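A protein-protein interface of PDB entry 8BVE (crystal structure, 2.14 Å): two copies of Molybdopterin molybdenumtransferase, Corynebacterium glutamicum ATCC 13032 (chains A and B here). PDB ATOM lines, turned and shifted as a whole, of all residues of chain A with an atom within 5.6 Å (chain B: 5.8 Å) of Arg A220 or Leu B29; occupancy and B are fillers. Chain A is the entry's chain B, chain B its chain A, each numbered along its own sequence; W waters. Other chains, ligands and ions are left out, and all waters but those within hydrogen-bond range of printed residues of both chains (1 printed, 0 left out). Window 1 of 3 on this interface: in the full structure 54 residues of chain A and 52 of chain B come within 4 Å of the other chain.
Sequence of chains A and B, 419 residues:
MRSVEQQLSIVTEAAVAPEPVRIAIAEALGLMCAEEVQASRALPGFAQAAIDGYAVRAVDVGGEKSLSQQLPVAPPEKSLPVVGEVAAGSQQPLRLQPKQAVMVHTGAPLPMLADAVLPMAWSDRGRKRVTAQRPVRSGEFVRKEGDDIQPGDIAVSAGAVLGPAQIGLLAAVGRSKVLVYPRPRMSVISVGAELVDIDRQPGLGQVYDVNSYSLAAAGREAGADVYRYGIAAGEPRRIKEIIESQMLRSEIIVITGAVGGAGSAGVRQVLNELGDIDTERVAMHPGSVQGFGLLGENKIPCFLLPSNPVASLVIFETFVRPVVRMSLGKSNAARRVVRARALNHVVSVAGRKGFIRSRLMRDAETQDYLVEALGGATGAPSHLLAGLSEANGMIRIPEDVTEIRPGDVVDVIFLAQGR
O of Val A226 lies within hydrogen-bond range of NH2 of Arg A220, at 3.4 Å.
Leu B29 touches Ala A217 (CD2 to O, 3.7 Å). Ala A217 touches Pro B164 (CB to CA, 3.7 Å). Ala A218 touches Pro B164 (N to CG, 3.6 Å). Leu B29 touches Arg A220 (CD2 to CB, 3.9 Å). Leu B29 touches Glu A221 (CD1 to OE2, 3.5 Å). Glu A221 touches Pro B164.
Of chain B, only Leu B29 comes within 4 Å of Arg A220. Printed residues of chain B within 4 Å of Glu A221: Leu B29 (3.5 Å) and Pro B164 (3.5 Å). Ile B25 touches none of the printed residues of chain A. Glu B27 touches none of the printed residues of chain A. Leu B29 touches just these residues of chain A: Ala A217, Arg A220 and Glu A221. Printed residues of chain A within 4 Å of Pro B164: Ala A217, Ala A218 and Glu A221. The nearest residue of chain B that does not touch Arg A220 is Ala B26 (4.7 Å). The nearest printed residue of chain B that does not touch Ala A217 is Ile B167 (4.5 Å).
Printed residues of chain B that touch a printed residue of chain A: Leu B29 and Pro B164. Hydrophobic or aromatic side chains of chain A within 4 Å of the printed part of chain B: Ala A217. Along chain A the printed residues that touch a printed residue of chain B span positions 217 to 221.
No position is printed for both chains.
Water W1 bridges the backbone carbonyl oxygen (O) of Ala B26 (2.8 Å) and the guanidinium group (NH1) of Arg A220 (2.9 Å).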
ATOM      1  N   LEU A 215      27.718   1.843  -9.341  1.00  0.00           N
ATOM      2  CA  LEU A 215      27.357   3.157  -9.867  1.00  0.00           C
ATOM      3  C   LEU A 215      26.025   3.648  -9.320  1.00  0.00           C
ATOM      4  O   LEU A 215      25.848   4.859  -9.136  1.00  0.00           O
ATOM      5  CB  LEU A 215      27.320   3.125 -11.393  1.00  0.00           C
ATOM      6  CG  LEU A 215      28.660   2.778 -12.036  1.00  0.00           C
ATOM      7  CD1 LEU A 215      28.517   2.754 -13.545  1.00  0.00           C
ATOM      8  CD2 LEU A 215      29.746   3.756 -11.606  1.00  0.00           C
ATOM      9  N   ALA A 216      25.085   2.742  -9.038  1.00  0.00           N
ATOM     10  CA  ALA A 216      23.882   3.162  -8.327  1.00  0.00           C
ATOM     11  C   ALA A 216      24.243   3.739  -6.965  1.00  0.00           C
ATOM     12  O   ALA A 216      23.690   4.763  -6.545  1.00  0.00           O
ATOM     13  CB  ALA A 216      22.907   1.993  -8.173  1.00  0.00           C
ATOM     14  N   ALA A 217      25.174   3.093  -6.262  1.00  0.00           N
ATOM     15  CA  ALA A 217      25.604   3.612  -4.970  1.00  0.00           C
ATOM     16  C   ALA A 217      26.283   4.967  -5.122  1.00  0.00           C
ATOM     17  O   ALA A 217      26.027   5.891  -4.342  1.00  0.00           O
ATOM     18  CB  ALA A 217      26.540   2.611  -4.289  1.00  0.00           C
ATOM     19  N   ALA A 218      27.145   5.112  -6.133  1.00  0.00           N
ATOM     20  CA  ALA A 218      27.796   6.397  -6.355  1.00  0.00           C
ATOM     21  C   ALA A 218      26.779   7.471  -6.713  1.00  0.00           C
ATOM     22  O   ALA A 218      26.951   8.636  -6.338  1.00  0.00           O
ATOM     23  CB  ALA A 218      28.861   6.273  -7.448  1.00  0.00           C
ATOM     24  N   GLY A 219      25.717   7.096  -7.427  1.00  0.00           N
ATOM     25  CA  GLY A 219      24.663   8.051  -7.730  1.00  0.00           C
ATOM     26  C   GLY A 219      23.899   8.495  -6.496  1.00  0.00           C
ATOM     27  O   GLY A 219      23.537   9.666  -6.369  1.00  0.00           O
ATOM     28  N   ARG A 220      23.638   7.570  -5.571  1.00  0.00           N
ATOM     29  CA  ARG A 220      22.951   7.960  -4.344  1.00  0.00           C
ATOM     30  C   ARG A 220      23.825   8.886  -3.506  1.00  0.00           C
ATOM     31  O   ARG A 220      23.346   9.903  -2.991  1.00  0.00           O
ATOM     32  CB  ARG A 220      22.538   6.722  -3.538  1.00  0.00           C
ATOM     33  CG  ARG A 220      21.546   5.820  -4.269  1.00  0.00           C
ATOM     34  CD  ARG A 220      20.754   4.891  -3.333  1.00  0.00           C
ATOM     35  NE  ARG A 220      19.778   4.124  -4.101  1.00  0.00           N
ATOM     36  CZ  ARG A 220      20.067   3.045  -4.815  1.00  0.00           C
ATOM     37  NH1 ARG A 220      21.279   2.514  -4.805  1.00  0.00           N
ATOM     38  NH2 ARG A 220      19.122   2.497  -5.578  1.00  0.00           N
ATOM     39  N   GLU A 221      25.118   8.567  -3.388  1.00  0.00           N
ATOM     40  CA  GLU A 221      26.028   9.425  -2.634  1.00  0.00           C
ATOM     41  C   GLU A 221      26.151  10.810  -3.261  1.00  0.00           C
ATOM     42  O   GLU A 221      26.297  11.803  -2.542  1.00  0.00           O
ATOM     43  CB  GLU A 221      27.394   8.741  -2.523  1.00  0.00           C
ATOM     44  CG  GLU A 221      27.735   8.322  -1.100  1.00  0.00           C
ATOM     45  CD  GLU A 221      29.086   7.633  -0.969  1.00  0.00           C
ATOM     46  OE1 GLU A 221      30.021   7.937  -1.746  1.00  0.00           O
ATOM     47  OE2 GLU A 221      29.211   6.787  -0.059  1.00  0.00           O
ATOM     48  N   ALA A 222      26.048  10.904  -4.591  1.00  0.00           N
ATOM     49  CA  ALA A 222      26.097  12.201  -5.260  1.00  0.00           C
ATOM     50  C   ALA A 222      24.838  13.028  -5.030  1.00  0.00           C
ATOM     51  O   ALA A 222      24.854  14.240  -5.274  1.00  0.00           O
ATOM     52  CB  ALA A 222      26.327  12.014  -6.761  1.00  0.00           C
ATOM     53  N   GLY A 223      23.747  12.409  -4.585  1.00  0.00           N
ATOM     54  CA  GLY A 223      22.518  13.125  -4.327  1.00  0.00           C
ATOM     55  C   GLY A 223      21.392  12.866  -5.304  1.00  0.00           C
ATOM     56  O   GLY A 223      20.374  13.561  -5.241  1.00  0.00           O
ATOM     57  N   ALA A 224      21.534  11.896  -6.196  1.00  0.00           N
ATOM     58  CA  ALA A 224      20.495  11.580  -7.160  1.00  0.00           C
ATOM     59  C   ALA A 224      19.475  10.622  -6.558  1.00  0.00           C
ATOM     60  O   ALA A 224      19.749   9.904  -5.593  1.00  0.00           O
ATOM     61  CB  ALA A 224      21.096  10.960  -8.423  1.00  0.00           C
ATOM     62  N   VAL A 226      18.043   7.423  -7.401  1.00  0.00           N
ATOM     63  CA  VAL A 226      18.617   6.412  -8.284  1.00  0.00           C
ATOM     64  C   VAL A 226      17.693   5.207  -8.363  1.00  0.00           C
ATOM     65  O   VAL A 226      17.251   4.683  -7.334  1.00  0.00           O
ATOM     66  CB  VAL A 226      20.016   5.985  -7.812  1.00  0.00           C
ATOM     67  CG1 VAL A 226      20.560   4.881  -8.720  1.00  0.00           C
ATOM     68  CG2 VAL A 226      20.961   7.179  -7.790  1.00  0.00           C
ATOM     69  N   TYR A 227      17.428   4.751  -9.584  1.00  0.00           N
ATOM     70  CA  TYR A 227      16.799   3.461  -9.831  1.00  0.00           C
ATOM     71  C   TYR A 227      17.803   2.589 -10.571  1.00  0.00           C
ATOM     72  O   TYR A 227      18.240   2.940 -11.671  1.00  0.00           O
ATOM     73  CB  TYR A 227      15.510   3.605 -10.642  1.00  0.00           C
ATOM     74  CG  TYR A 227      14.885   2.282 -11.021  1.00  0.00           C
ATOM     75  CD1 TYR A 227      14.156   1.542 -10.095  1.00  0.00           C
ATOM     76  CD2 TYR A 227      15.028   1.766 -12.305  1.00  0.00           C
ATOM     77  CE1 TYR A 227      13.585   0.326 -10.438  1.00  0.00           C
ATOM     78  CE2 TYR A 227      14.463   0.554 -12.657  1.00  0.00           C
ATOM     79  CZ  TYR A 227      13.745  -0.161 -11.723  1.00  0.00           C
ATOM     80  OH  TYR A 227      13.184  -1.366 -12.078  1.00  0.00           O
ATOM     81  N   ARG A 228      18.184   1.471  -9.953  1.00  0.00           N
ATOM     82  CA  ARG A 228      19.122   0.526 -10.558  1.00  0.00           C
ATOM     83  C   ARG A 228      18.319  -0.469 -11.385  1.00  0.00           C
ATOM     84  O   ARG A 228      17.691  -1.382 -10.844  1.00  0.00           O
ATOM     85  CB  ARG A 228      19.954  -0.175  -9.487  1.00  0.00           C
ATOM     86  CG  ARG A 228      21.125  -0.998 -10.043  1.00  0.00           C
ATOM     87  CD  ARG A 228      21.794  -1.836  -8.956  1.00  0.00           C
ATOM     88  NE  ARG A 228      20.884  -2.828  -8.394  1.00  0.00           N
ATOM     89  CZ  ARG A 228      20.655  -4.022  -8.923  1.00  0.00           C
ATOM     90  NH1 ARG A 228      21.278  -4.422 -10.025  1.00  0.00           N
ATOM     91  NH2 ARG A 228      19.781  -4.838  -8.329  1.00  0.00           N
ATOM     92  N   ILE B  25      23.068  -5.831  -0.375  1.00  0.00           N
ATOM     93  CA  ILE B  25      24.266  -4.988  -0.409  1.00  0.00           C
ATOM     94  C   ILE B  25      23.936  -3.562  -0.836  1.00  0.00           C
ATOM     95  O   ILE B  25      24.548  -2.608  -0.340  1.00  0.00           O
ATOM     96  CB  ILE B  25      25.362  -5.611  -1.307  1.00  0.00           C
ATOM     97  CG1 ILE B  25      24.871  -5.831  -2.744  1.00  0.00           C
ATOM     98  CG2 ILE B  25      25.873  -6.911  -0.705  1.00  0.00           C
ATOM     99  CD1 ILE B  25      26.002  -6.176  -3.718  1.00  0.00           C
ATOM    100  N   ALA B  26      22.951  -3.377  -1.722  1.00  0.00           N
ATOM    101  CA  ALA B  26      22.611  -2.018  -2.145  1.00  0.00           C
ATOM    102  C   ALA B  26      22.119  -1.175  -0.975  1.00  0.00           C
ATOM    103  O   ALA B  26      22.360   0.040  -0.934  1.00  0.00           O
ATOM    104  CB  ALA B  26      21.557  -2.042  -3.254  1.00  0.00           C
ATOM    105  N   GLU B  27      21.448  -1.802  -0.010  1.00  0.00           N
ATOM    106  CA  GLU B  27      20.931  -1.101   1.157  1.00  0.00           C
ATOM    107  C   GLU B  27      21.994  -0.849   2.212  1.00  0.00           C
ATOM    108  O   GLU B  27      21.696  -0.203   3.222  1.00  0.00           O
ATOM    109  CB  GLU B  27      19.773  -1.891   1.772  1.00  0.00           C
ATOM    110  CG  GLU B  27      18.631  -2.169   0.807  1.00  0.00           C
ATOM    111  CD  GLU B  27      17.584  -3.081   1.401  1.00  0.00           C
ATOM    112  OE1 GLU B  27      17.344  -2.984   2.625  1.00  0.00           O
ATOM    113  OE2 GLU B  27      17.000  -3.893   0.649  1.00  0.00           O
ATOM    114  N   ALA B  28      23.217  -1.337   2.010  1.00  0.00           N
ATOM    115  CA  ALA B  28      24.277  -1.193   3.000  1.00  0.00           C
ATOM    116  C   ALA B  28      25.126   0.054   2.803  1.00  0.00           C
ATOM    117  O   ALA B  28      26.088   0.248   3.552  1.00  0.00           O
ATOM    118  CB  ALA B  28      25.177  -2.434   2.988  1.00  0.00           C
ATOM    119  N   LEU B  29      24.781   0.912   1.843  1.00  0.00           N
ATOM    120  CA  LEU B  29      25.615   2.063   1.517  1.00  0.00           C
ATOM    121  C   LEU B  29      25.787   2.992   2.716  1.00  0.00           C
ATOM    122  O   LEU B  29      24.807   3.429   3.327  1.00  0.00           O
ATOM    123  CB  LEU B  29      25.002   2.832   0.348  1.00  0.00           C
ATOM    124  CG  LEU B  29      25.629   4.199   0.065  1.00  0.00           C
ATOM    125  CD1 LEU B  29      27.079   4.027  -0.375  1.00  0.00           C
ATOM    126  CD2 LEU B  29      24.823   4.968  -0.980  1.00  0.00           C
ATOM    127  N   GLY B  30      27.043   3.309   3.038  1.00  0.00           N
ATOM    128  CA  GLY B  30      27.341   4.204   4.137  1.00  0.00           C
ATOM    129  C   GLY B  30      27.307   3.572   5.512  1.00  0.00           C
ATOM    130  O   GLY B  30      27.541   4.273   6.504  1.00  0.00           O
ATOM    131  N   LEU B  31      27.013   2.282   5.609  1.00  0.00           N
ATOM    132  CA  LEU B  31      27.007   1.583   6.885  1.00  0.00           C
ATOM    133  C   LEU B  31      28.334   0.864   7.102  1.00  0.00           C
ATOM    134  O   LEU B  31      29.051   0.529   6.157  1.00  0.00           O
ATOM    135  CB  LEU B  31      25.850   0.580   6.952  1.00  0.00           C
ATOM    136  CG  LEU B  31      24.451   1.146   6.700  1.00  0.00           C
ATOM    137  CD1 LEU B  31      23.373   0.109   7.023  1.00  0.00           C
ATOM    138  CD2 LEU B  31      24.236   2.415   7.519  1.00  0.00           C
ATOM    139  N   LEU B 162      30.964   0.935   4.071  1.00  0.00           N
ATOM    140  CA  LEU B 162      30.663   0.404   2.744  1.00  0.00           C
ATOM    141  C   LEU B 162      30.276   1.556   1.824  1.00  0.00           C
ATOM    142  O   LEU B 162      29.126   2.001   1.817  1.00  0.00           O
ATOM    143  CB  LEU B 162      29.554  -0.638   2.834  1.00  0.00           C
ATOM    144  CG  LEU B 162      29.939  -1.892   3.625  1.00  0.00           C
ATOM    145  CD1 LEU B 162      28.762  -2.832   3.736  1.00  0.00           C
ATOM    146  CD2 LEU B 162      31.139  -2.595   2.984  1.00  0.00           C
ATOM    147  N   GLY B 163      31.236   2.022   1.027  1.00  0.00           N
ATOM    148  CA  GLY B 163      30.978   3.011   0.007  1.00  0.00           C
ATOM    149  C   GLY B 163      30.718   2.326  -1.320  1.00  0.00           C
ATOM    150  O   GLY B 163      30.672   1.094  -1.401  1.00  0.00           O
ATOM    151  N   PRO B 164      30.547   3.108  -2.391  1.00  0.00           N
ATOM    152  CA  PRO B 164      30.237   2.493  -3.695  1.00  0.00           C
ATOM    153  C   PRO B 164      31.274   1.484  -4.171  1.00  0.00           C
ATOM    154  O   PRO B 164      30.893   0.448  -4.729  1.00  0.00           O
ATOM    155  CB  PRO B 164      30.135   3.701  -4.638  1.00  0.00           C
ATOM    156  CG  PRO B 164      29.796   4.851  -3.741  1.00  0.00           C
ATOM    157  CD  PRO B 164      30.482   4.579  -2.435  1.00  0.00           C
ATOM    158  N   ILE B 167      30.718  -1.751  -2.293  1.00  0.00           N
ATOM    159  CA  ILE B 167      29.530  -2.427  -2.808  1.00  0.00           C
ATOM    160  C   ILE B 167      29.863  -3.142  -4.113  1.00  0.00           C
ATOM    161  O   ILE B 167      29.431  -4.276  -4.346  1.00  0.00           O
ATOM    162  CB  ILE B 167      28.373  -1.426  -3.004  1.00  0.00           C
ATOM    163  CG1 ILE B 167      28.003  -0.724  -1.689  1.00  0.00           C
ATOM    164  CG2 ILE B 167      27.157  -2.117  -3.616  1.00  0.00           C
ATOM    165  CD1 ILE B 167      27.536  -1.652  -0.602  1.00  0.00           C
ATOM    166  N   ARG B 183      21.744   1.474  11.378  1.00  0.00           N
ATOM    167  CA  ARG B 183      21.442   2.737  12.030  1.00  0.00           C
ATOM    168  C   ARG B 183      20.523   2.487  13.223  1.00  0.00           C
ATOM    169  O   ARG B 183      19.643   1.621  13.158  1.00  0.00           O
ATOM    170  CB  ARG B 183      20.777   3.707  11.048  1.00  0.00           C
ATOM    171  CG  ARG B 183      21.704   4.151   9.925  1.00  0.00           C
ATOM    172  CD  ARG B 183      21.034   5.110   8.944  1.00  0.00           C
ATOM    173  NE  ARG B 183      21.970   5.473   7.884  1.00  0.00           N
ATOM    174  CZ  ARG B 183      22.962   6.345   8.026  1.00  0.00           C
ATOM    175  NH1 ARG B 183      23.123   7.027   9.151  1.00  0.00           N
ATOM    176  NH2 ARG B 183      23.819   6.529   7.020  1.00  0.00           N
HETATM  177  O   HOH W   1      23.424   1.630  -3.010  1.00  0.00           O
